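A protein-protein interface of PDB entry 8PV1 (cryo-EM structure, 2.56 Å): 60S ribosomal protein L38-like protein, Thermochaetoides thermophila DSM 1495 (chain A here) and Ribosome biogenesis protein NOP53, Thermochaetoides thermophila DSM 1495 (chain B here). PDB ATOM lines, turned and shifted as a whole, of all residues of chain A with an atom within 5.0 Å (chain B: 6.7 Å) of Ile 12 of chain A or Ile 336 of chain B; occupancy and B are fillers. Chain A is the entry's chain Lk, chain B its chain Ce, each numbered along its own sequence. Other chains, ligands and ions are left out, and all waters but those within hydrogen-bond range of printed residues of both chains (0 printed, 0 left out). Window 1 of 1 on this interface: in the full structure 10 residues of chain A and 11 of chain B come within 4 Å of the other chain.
Hydrophobic or aromatic side chains of chain B that line the printed part of chain A: Ile 336, Ala 337 and Val 340.
Along chain B the printed residues that touch a printed residue of chain A span positions 329 to 344.
Of the 11 printed residues of chain A, 5 touch a printed residue of chain B.
Among the printed residues, 9 pairs touch across the chains.
Among the printed residues, Asp or Glu carboxylates within 4 Å of a Lys or Arg side-chain nitrogen of the other chain: Lys 9 of chain A with Glu 339 of chain B and Arg 16 of chain A with Glu 344 of chain B.
The side-chain carboxylate (OE1) of Glu 344 of chain B is in salt-bridge range of the guanidinium group (NH2) of Arg 16 of chain A, at 2.6 Å.
The side-chain amino group of Lys 9 of chain A lies within salt-bridge range of the side-chain carboxylate of Glu 339 of chain B (3.3 Å).
N of Ile 8 of chain A lies within hydrogen-bond range of OE1 of Gln 329 of chain B, at 3.3 Å.
Ile 336 of chain B touches just these residues of chain A: Lys 9 (3.7 Å) and Ile 12 (3.9 Å).
Printed residues of chain A within 4 Å of Leu 330 of chain B: Ile 8.
Printed residues of chain A within 4 Å of Glu 344 of chain B: Arg 16.
Phe 11 of chain A touches none of the printed residues of chain B.
The nearest printed residue of chain A that does not touch Ala 333 of chain B is Ile 12 of chain A (4.1 Å).
Ile 8 of chain A touches Leu 330 of chain B.
CA of Lys 9 of chain A touches CG2 of Ile 336 of chain B, 3.7 Å away.
Ile 12 of chain A touches Ile 336 of chain B (CD1 to CG2, 3.9 Å).
CG1 of Val 340 of chain B touches CD of Arg 16 of chain A (3.7 Å).
OG of Ser 74 of chain A touches O of Ala 333 of chain B (3.9 Å).
Ser 74 of chain A touches Ala 337 of chain B (OG to CB, 3.4 Å).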
ATOM      1  N   ILE A   8     -14.208  -1.865 -19.745  1.00  0.00           N
ATOM      2  CA  ILE A   8     -13.555  -2.174 -18.475  1.00  0.00           C
ATOM      3  C   ILE A   8     -13.187  -3.650 -18.408  1.00  0.00           C
ATOM      4  O   ILE A   8     -12.123  -4.016 -17.895  1.00  0.00           O
ATOM      5  CB  ILE A   8     -14.459  -1.755 -17.300  1.00  0.00           C
ATOM      6  CG1 ILE A   8     -14.861  -0.285 -17.432  1.00  0.00           C
ATOM      7  CG2 ILE A   8     -13.770  -1.998 -15.966  1.00  0.00           C
ATOM      8  CD1 ILE A   8     -13.726   0.683 -17.216  1.00  0.00           C
ATOM      9  N   LYS A   9     -14.053  -4.518 -18.939  1.00  0.00           N
ATOM     10  CA  LYS A   9     -13.773  -5.950 -18.932  1.00  0.00           C
ATOM     11  C   LYS A   9     -12.554  -6.285 -19.780  1.00  0.00           C
ATOM     12  O   LYS A   9     -11.675  -7.044 -19.347  1.00  0.00           O
ATOM     13  CB  LYS A   9     -14.997  -6.719 -19.424  1.00  0.00           C
ATOM     14  CG  LYS A   9     -14.850  -8.226 -19.352  1.00  0.00           C
ATOM     15  CD  LYS A   9     -16.128  -8.921 -19.775  1.00  0.00           C
ATOM     16  CE  LYS A   9     -15.979 -10.428 -19.710  1.00  0.00           C
ATOM     17  NZ  LYS A   9     -17.226 -11.125 -20.125  1.00  0.00           N
ATOM     18  N   LYS A  10     -12.471  -5.708 -20.982  1.00  0.00           N
ATOM     19  CA  LYS A  10     -11.320  -5.960 -21.841  1.00  0.00           C
ATOM     20  C   LYS A  10     -10.053  -5.370 -21.236  1.00  0.00           C
ATOM     21  O   LYS A  10      -8.974  -5.961 -21.350  1.00  0.00           O
ATOM     22  CB  LYS A  10     -11.572  -5.405 -23.245  1.00  0.00           C
ATOM     23  CG  LYS A  10     -10.439  -5.661 -24.229  1.00  0.00           C
ATOM     24  CD  LYS A  10     -10.790  -5.213 -25.640  1.00  0.00           C
ATOM     25  CE  LYS A  10     -10.785  -3.701 -25.767  1.00  0.00           C
ATOM     26  NZ  LYS A  10     -11.011  -3.249 -27.165  1.00  0.00           N
ATOM     27  N   PHE A  11     -10.171  -4.229 -20.550  1.00  0.00           N
ATOM     28  CA  PHE A  11      -9.016  -3.662 -19.860  1.00  0.00           C
ATOM     29  C   PHE A  11      -8.536  -4.569 -18.730  1.00  0.00           C
ATOM     30  O   PHE A  11      -7.327  -4.714 -18.514  1.00  0.00           O
ATOM     31  CB  PHE A  11      -9.346  -2.274 -19.320  1.00  0.00           C
ATOM     32  CG  PHE A  11      -8.155  -1.548 -18.780  1.00  0.00           C
ATOM     33  CD1 PHE A  11      -7.231  -0.977 -19.638  1.00  0.00           C
ATOM     34  CD2 PHE A  11      -7.946  -1.451 -17.416  1.00  0.00           C
ATOM     35  CE1 PHE A  11      -6.126  -0.317 -19.146  1.00  0.00           C
ATOM     36  CE2 PHE A  11      -6.845  -0.790 -16.918  1.00  0.00           C
ATOM     37  CZ  PHE A  11      -5.933  -0.226 -17.785  1.00  0.00           C
ATOM     38  N   ILE A  12      -9.469  -5.183 -17.999  1.00  0.00           N
ATOM     39  CA  ILE A  12      -9.097  -6.105 -16.926  1.00  0.00           C
ATOM     40  C   ILE A  12      -8.403  -7.340 -17.494  1.00  0.00           C
ATOM     41  O   ILE A  12      -7.400  -7.812 -16.943  1.00  0.00           O
ATOM     42  CB  ILE A  12     -10.334  -6.467 -16.080  1.00  0.00           C
ATOM     43  CG1 ILE A  12     -10.769  -5.264 -15.243  1.00  0.00           C
ATOM     44  CG2 ILE A  12     -10.056  -7.647 -15.163  1.00  0.00           C
ATOM     45  CD1 ILE A  12     -12.015  -5.504 -14.430  1.00  0.00           C
ATOM     46  N   GLU A  13      -8.908  -7.869 -18.615  1.00  0.00           N
ATOM     47  CA  GLU A  13      -8.238  -9.009 -19.248  1.00  0.00           C
ATOM     48  C   GLU A  13      -6.850  -8.637 -19.766  1.00  0.00           C
ATOM     49  O   GLU A  13      -5.910  -9.439 -19.671  1.00  0.00           O
ATOM     50  CB  GLU A  13      -9.089  -9.587 -20.377  1.00  0.00           C
ATOM     51  CG  GLU A  13     -10.509  -9.940 -19.987  1.00  0.00           C
ATOM     52  CD  GLU A  13     -11.443  -9.986 -21.180  1.00  0.00           C
ATOM     53  OE1 GLU A  13     -11.283 -10.890 -22.026  1.00  0.00           O
ATOM     54  OE2 GLU A  13     -12.336  -9.120 -21.278  1.00  0.00           O
ATOM     55  N   ILE A  14      -6.700  -7.430 -20.318  1.00  0.00           N
ATOM     56  CA  ILE A  14      -5.387  -6.976 -20.777  1.00  0.00           C
ATOM     57  C   ILE A  14      -4.421  -6.857 -19.603  1.00  0.00           C
ATOM     58  O   ILE A  14      -3.258  -7.269 -19.695  1.00  0.00           O
ATOM     59  CB  ILE A  14      -5.515  -5.651 -21.555  1.00  0.00           C
ATOM     60  CG1 ILE A  14      -6.198  -5.879 -22.903  1.00  0.00           C
ATOM     61  CG2 ILE A  14      -4.160  -5.032 -21.798  1.00  0.00           C
ATOM     62  CD1 ILE A  14      -6.505  -4.603 -23.651  1.00  0.00           C
ATOM     63  N   CYS A  15      -4.889  -6.316 -18.476  1.00  0.00           N
ATOM     64  CA  CYS A  15      -4.038  -6.225 -17.295  1.00  0.00           C
ATOM     65  C   CYS A  15      -3.725  -7.588 -16.693  1.00  0.00           C
ATOM     66  O   CYS A  15      -2.682  -7.740 -16.049  1.00  0.00           O
ATOM     67  CB  CYS A  15      -4.684  -5.331 -16.238  1.00  0.00           C
ATOM     68  SG  CYS A  15      -4.746  -3.588 -16.683  1.00  0.00           S
ATOM     69  N   ARG A  16      -4.596  -8.574 -16.881  1.00  0.00           N
ATOM     70  CA  ARG A  16      -4.336  -9.926 -16.404  1.00  0.00           C
ATOM     71  C   ARG A  16      -3.507 -10.752 -17.379  1.00  0.00           C
ATOM     72  O   ARG A  16      -3.093 -11.861 -17.027  1.00  0.00           O
ATOM     73  CB  ARG A  16      -5.652 -10.648 -16.108  1.00  0.00           C
ATOM     74  CG  ARG A  16      -6.218 -10.326 -14.740  1.00  0.00           C
ATOM     75  CD  ARG A  16      -7.562 -11.007 -14.500  1.00  0.00           C
ATOM     76  NE  ARG A  16      -7.462 -12.395 -14.054  1.00  0.00           N
ATOM     77  CZ  ARG A  16      -6.878 -12.823 -12.939  1.00  0.00           C
ATOM     78  NH1 ARG A  16      -6.407 -11.985 -12.027  1.00  0.00           N
ATOM     79  NH2 ARG A  16      -6.797 -14.131 -12.713  1.00  0.00           N
ATOM     80  N   SER A  74      -9.184  -3.345  -8.060  1.00  0.00           N
ATOM     81  CA  SER A  74      -9.655  -4.360  -8.991  1.00  0.00           C
ATOM     82  C   SER A  74      -8.570  -4.814  -9.955  1.00  0.00           C
ATOM     83  O   SER A  74      -8.632  -5.942 -10.452  1.00  0.00           O
ATOM     84  CB  SER A  74     -10.860  -3.840  -9.777  1.00  0.00           C
ATOM     85  OG  SER A  74     -11.311  -4.805 -10.710  1.00  0.00           O
ATOM     86  N   LEU A  75      -7.595  -3.961 -10.237  1.00  0.00           N
ATOM     87  CA  LEU A  75      -6.447  -4.359 -11.041  1.00  0.00           C
ATOM     88  C   LEU A  75      -5.596  -5.376 -10.285  1.00  0.00           C
ATOM     89  O   LEU A  75      -5.594  -5.394  -9.051  1.00  0.00           O
ATOM     90  CB  LEU A  75      -5.617  -3.129 -11.411  1.00  0.00           C
ATOM     91  CG  LEU A  75      -6.316  -2.137 -12.344  1.00  0.00           C
ATOM     92  CD1 LEU A  75      -5.407  -0.966 -12.675  1.00  0.00           C
ATOM     93  CD2 LEU A  75      -6.794  -2.830 -13.609  1.00  0.00           C
ATOM     94  N   GLN B 328     -21.114   2.809 -16.164  1.00  0.00           N
ATOM     95  CA  GLN B 328     -21.826   1.728 -15.480  1.00  0.00           C
ATOM     96  C   GLN B 328     -20.929   0.509 -15.277  1.00  0.00           C
ATOM     97  O   GLN B 328     -20.994  -0.160 -14.237  1.00  0.00           O
ATOM     98  CB  GLN B 328     -23.085   1.353 -16.262  1.00  0.00           C
ATOM     99  CG  GLN B 328     -24.195   2.386 -16.139  1.00  0.00           C
ATOM    100  CD  GLN B 328     -25.306   2.187 -17.154  1.00  0.00           C
ATOM    101  OE1 GLN B 328     -25.517   1.083 -17.654  1.00  0.00           O
ATOM    102  NE2 GLN B 328     -26.012   3.266 -17.476  1.00  0.00           N
ATOM    103  N   GLN B 329     -20.090   0.199 -16.269  1.00  0.00           N
ATOM    104  CA  GLN B 329     -19.118  -0.882 -16.097  1.00  0.00           C
ATOM    105  C   GLN B 329     -18.093  -0.549 -15.012  1.00  0.00           C
ATOM    106  O   GLN B 329     -17.694  -1.427 -14.233  1.00  0.00           O
ATOM    107  CB  GLN B 329     -18.427  -1.179 -17.424  1.00  0.00           C
ATOM    108  CG  GLN B 329     -19.360  -1.656 -18.508  1.00  0.00           C
ATOM    109  CD  GLN B 329     -18.656  -1.839 -19.836  1.00  0.00           C
ATOM    110  OE1 GLN B 329     -17.459  -1.573 -19.965  1.00  0.00           O
ATOM    111  NE2 GLN B 329     -19.403  -2.279 -20.839  1.00  0.00           N
ATOM    112  N   LEU B 330     -17.661   0.718 -14.943  1.00  0.00           N
ATOM    113  CA  LEU B 330     -16.779   1.147 -13.856  1.00  0.00           C
ATOM    114  C   LEU B 330     -17.468   1.004 -12.497  1.00  0.00           C
ATOM    115  O   LEU B 330     -16.819   0.672 -11.500  1.00  0.00           O
ATOM    116  CB  LEU B 330     -16.322   2.589 -14.079  1.00  0.00           C
ATOM    117  CG  LEU B 330     -15.399   3.189 -13.015  1.00  0.00           C
ATOM    118  CD1 LEU B 330     -14.083   2.406 -12.966  1.00  0.00           C
ATOM    119  CD2 LEU B 330     -15.150   4.654 -13.299  1.00  0.00           C
ATOM    120  N   GLN B 332     -19.749  -1.368 -11.857  1.00  0.00           N
ATOM    121  CA  GLN B 332     -19.787  -2.806 -11.613  1.00  0.00           C
ATOM    122  C   GLN B 332     -18.435  -3.470 -11.865  1.00  0.00           C
ATOM    123  O   GLN B 332     -18.381  -4.621 -12.307  1.00  0.00           O
ATOM    124  CB  GLN B 332     -20.869  -3.471 -12.461  1.00  0.00           C
ATOM    125  CG  GLN B 332     -22.248  -2.849 -12.328  1.00  0.00           C
ATOM    126  CD  GLN B 332     -22.844  -3.004 -10.949  1.00  0.00           C
ATOM    127  OE1 GLN B 332     -22.618  -4.006 -10.275  1.00  0.00           O
ATOM    128  NE2 GLN B 332     -23.613  -2.009 -10.521  1.00  0.00           N
ATOM    129  N   ALA B 333     -17.341  -2.751 -11.585  1.00  0.00           N
ATOM    130  CA  ALA B 333     -15.991  -3.240 -11.878  1.00  0.00           C
ATOM    131  C   ALA B 333     -15.639  -4.524 -11.127  1.00  0.00           C
ATOM    132  O   ALA B 333     -15.016  -5.423 -11.703  1.00  0.00           O
ATOM    133  CB  ALA B 333     -14.964  -2.153 -11.556  1.00  0.00           C
ATOM    134  N   LYS B 334     -15.996  -4.622  -9.838  1.00  0.00           N
ATOM    135  CA  LYS B 334     -15.574  -5.775  -9.037  1.00  0.00           C
ATOM    136  C   LYS B 334     -16.219  -7.071  -9.509  1.00  0.00           C
ATOM    137  O   LYS B 334     -15.570  -8.127  -9.518  1.00  0.00           O
ATOM    138  CB  LYS B 334     -15.880  -5.560  -7.555  1.00  0.00           C
ATOM    139  CG  LYS B 334     -14.743  -4.943  -6.761  1.00  0.00           C
ATOM    140  CD  LYS B 334     -15.065  -4.913  -5.270  1.00  0.00           C
ATOM    141  CE  LYS B 334     -13.907  -4.360  -4.457  1.00  0.00           C
ATOM    142  NZ  LYS B 334     -12.780  -5.326  -4.373  1.00  0.00           N
ATOM    143  N   LYS B 335     -17.499  -7.014  -9.877  1.00  0.00           N
ATOM    144  CA  LYS B 335     -18.178  -8.187 -10.412  1.00  0.00           C
ATOM    145  C   LYS B 335     -17.519  -8.649 -11.706  1.00  0.00           C
ATOM    146  O   LYS B 335     -17.386  -9.852 -11.956  1.00  0.00           O
ATOM    147  CB  LYS B 335     -19.656  -7.867 -10.633  1.00  0.00           C
ATOM    148  CG  LYS B 335     -20.479  -9.028 -11.153  1.00  0.00           C
ATOM    149  CD  LYS B 335     -21.953  -8.667 -11.206  1.00  0.00           C
ATOM    150  CE  LYS B 335     -22.240  -7.676 -12.322  1.00  0.00           C
ATOM    151  NZ  LYS B 335     -22.059  -8.276 -13.674  1.00  0.00           N
ATOM    152  N   ILE B 336     -17.068  -7.693 -12.521  1.00  0.00           N
ATOM    153  CA  ILE B 336     -16.362  -8.011 -13.758  1.00  0.00           C
ATOM    154  C   ILE B 336     -15.040  -8.713 -13.465  1.00  0.00           C
ATOM    155  O   ILE B 336     -14.686  -9.696 -14.127  1.00  0.00           O
ATOM    156  CB  ILE B 336     -16.157  -6.731 -14.588  1.00  0.00           C
ATOM    157  CG1 ILE B 336     -17.506  -6.147 -15.007  1.00  0.00           C
ATOM    158  CG2 ILE B 336     -15.303  -7.011 -15.791  1.00  0.00           C
ATOM    159  CD1 ILE B 336     -17.410  -4.763 -15.598  1.00  0.00           C
ATOM    160  N   ALA B 337     -14.292  -8.223 -12.472  1.00  0.00           N
ATOM    161  CA  ALA B 337     -13.019  -8.849 -12.120  1.00  0.00           C
ATOM    162  C   ALA B 337     -13.222 -10.264 -11.592  1.00  0.00           C
ATOM    163  O   ALA B 337     -12.464 -11.181 -11.941  1.00  0.00           O
ATOM    164  CB  ALA B 337     -12.281  -7.995 -11.091  1.00  0.00           C
ATOM    165  N   ALA B 338     -14.251 -10.461 -10.761  1.00  0.00           N
ATOM    166  CA  ALA B 338     -14.565 -11.799 -10.270  1.00  0.00           C
ATOM    167  C   ALA B 338     -14.970 -12.729 -11.409  1.00  0.00           C
ATOM    168  O   ALA B 338     -14.574 -13.900 -11.434  1.00  0.00           O
ATOM    169  CB  ALA B 338     -15.671 -11.724  -9.218  1.00  0.00           C
ATOM    170  N   GLU B 339     -15.749 -12.218 -12.368  1.00  0.00           N
ATOM    171  CA  GLU B 339     -16.163 -13.031 -13.509  1.00  0.00           C
ATOM    172  C   GLU B 339     -14.974 -13.410 -14.386  1.00  0.00           C
ATOM    173  O   GLU B 339     -14.899 -14.540 -14.882  1.00  0.00           O
ATOM    174  CB  GLU B 339     -17.221 -12.281 -14.321  1.00  0.00           C
ATOM    175  CG  GLU B 339     -17.992 -13.143 -15.316  1.00  0.00           C
ATOM    176  CD  GLU B 339     -17.319 -13.231 -16.671  1.00  0.00           C
ATOM    177  OE1 GLU B 339     -16.625 -12.267 -17.053  1.00  0.00           O
ATOM    178  OE2 GLU B 339     -17.484 -14.264 -17.354  1.00  0.00           O
ATOM    179  N   VAL B 340     -14.040 -12.478 -14.591  1.00  0.00           N
ATOM    180  CA  VAL B 340     -12.858 -12.761 -15.407  1.00  0.00           C
ATOM    181  C   VAL B 340     -11.973 -13.797 -14.719  1.00  0.00           C
ATOM    182  O   VAL B 340     -11.455 -14.723 -15.360  1.00  0.00           O
ATOM    183  CB  VAL B 340     -12.092 -11.457 -15.709  1.00  0.00           C
ATOM    184  CG1 VAL B 340     -10.726 -11.750 -16.303  1.00  0.00           C
ATOM    185  CG2 VAL B 340     -12.887 -10.594 -16.672  1.00  0.00           C
ATOM    186  N   GLU B 341     -11.807 -13.669 -13.398  1.00  0.00           N
ATOM    187  CA  GLU B 341     -11.029 -14.657 -12.653  1.00  0.00           C
ATOM    188  C   GLU B 341     -11.695 -16.030 -12.687  1.00  0.00           C
ATOM    189  O   GLU B 341     -11.014 -17.054 -12.819  1.00  0.00           O
ATOM    190  CB  GLU B 341     -10.825 -14.185 -11.214  1.00  0.00           C
ATOM    191  CG  GLU B 341     -10.001 -15.133 -10.361  1.00  0.00           C
ATOM    192  CD  GLU B 341      -9.501 -14.487  -9.085  1.00  0.00           C
ATOM    193  OE1 GLU B 341      -9.573 -13.244  -8.978  1.00  0.00           O
ATOM    194  OE2 GLU B 341      -9.035 -15.221  -8.189  1.00  0.00           O
ATOM    195  N   GLU B 344     -11.074 -17.535 -16.150  1.00  0.00           N
ATOM    196  CA  GLU B 344      -9.713 -18.052 -16.250  1.00  0.00           C
ATOM    197  C   GLU B 344      -9.554 -19.341 -15.452  1.00  0.00           C
ATOM    198  O   GLU B 344      -8.834 -20.255 -15.869  1.00  0.00           O
ATOM    199  CB  GLU B 344      -8.706 -16.999 -15.786  1.00  0.00           C
ATOM    200  CG  GLU B 344      -8.537 -15.843 -16.756  1.00  0.00           C
ATOM    201  CD  GLU B 344      -7.463 -14.870 -16.316  1.00  0.00           C
ATOM    202  OE1 GLU B 344      -7.000 -14.978 -15.163  1.00  0.00           O
ATOM    203  OE2 GLU B 344      -7.078 -14.000 -17.126  1.00  0.00           O
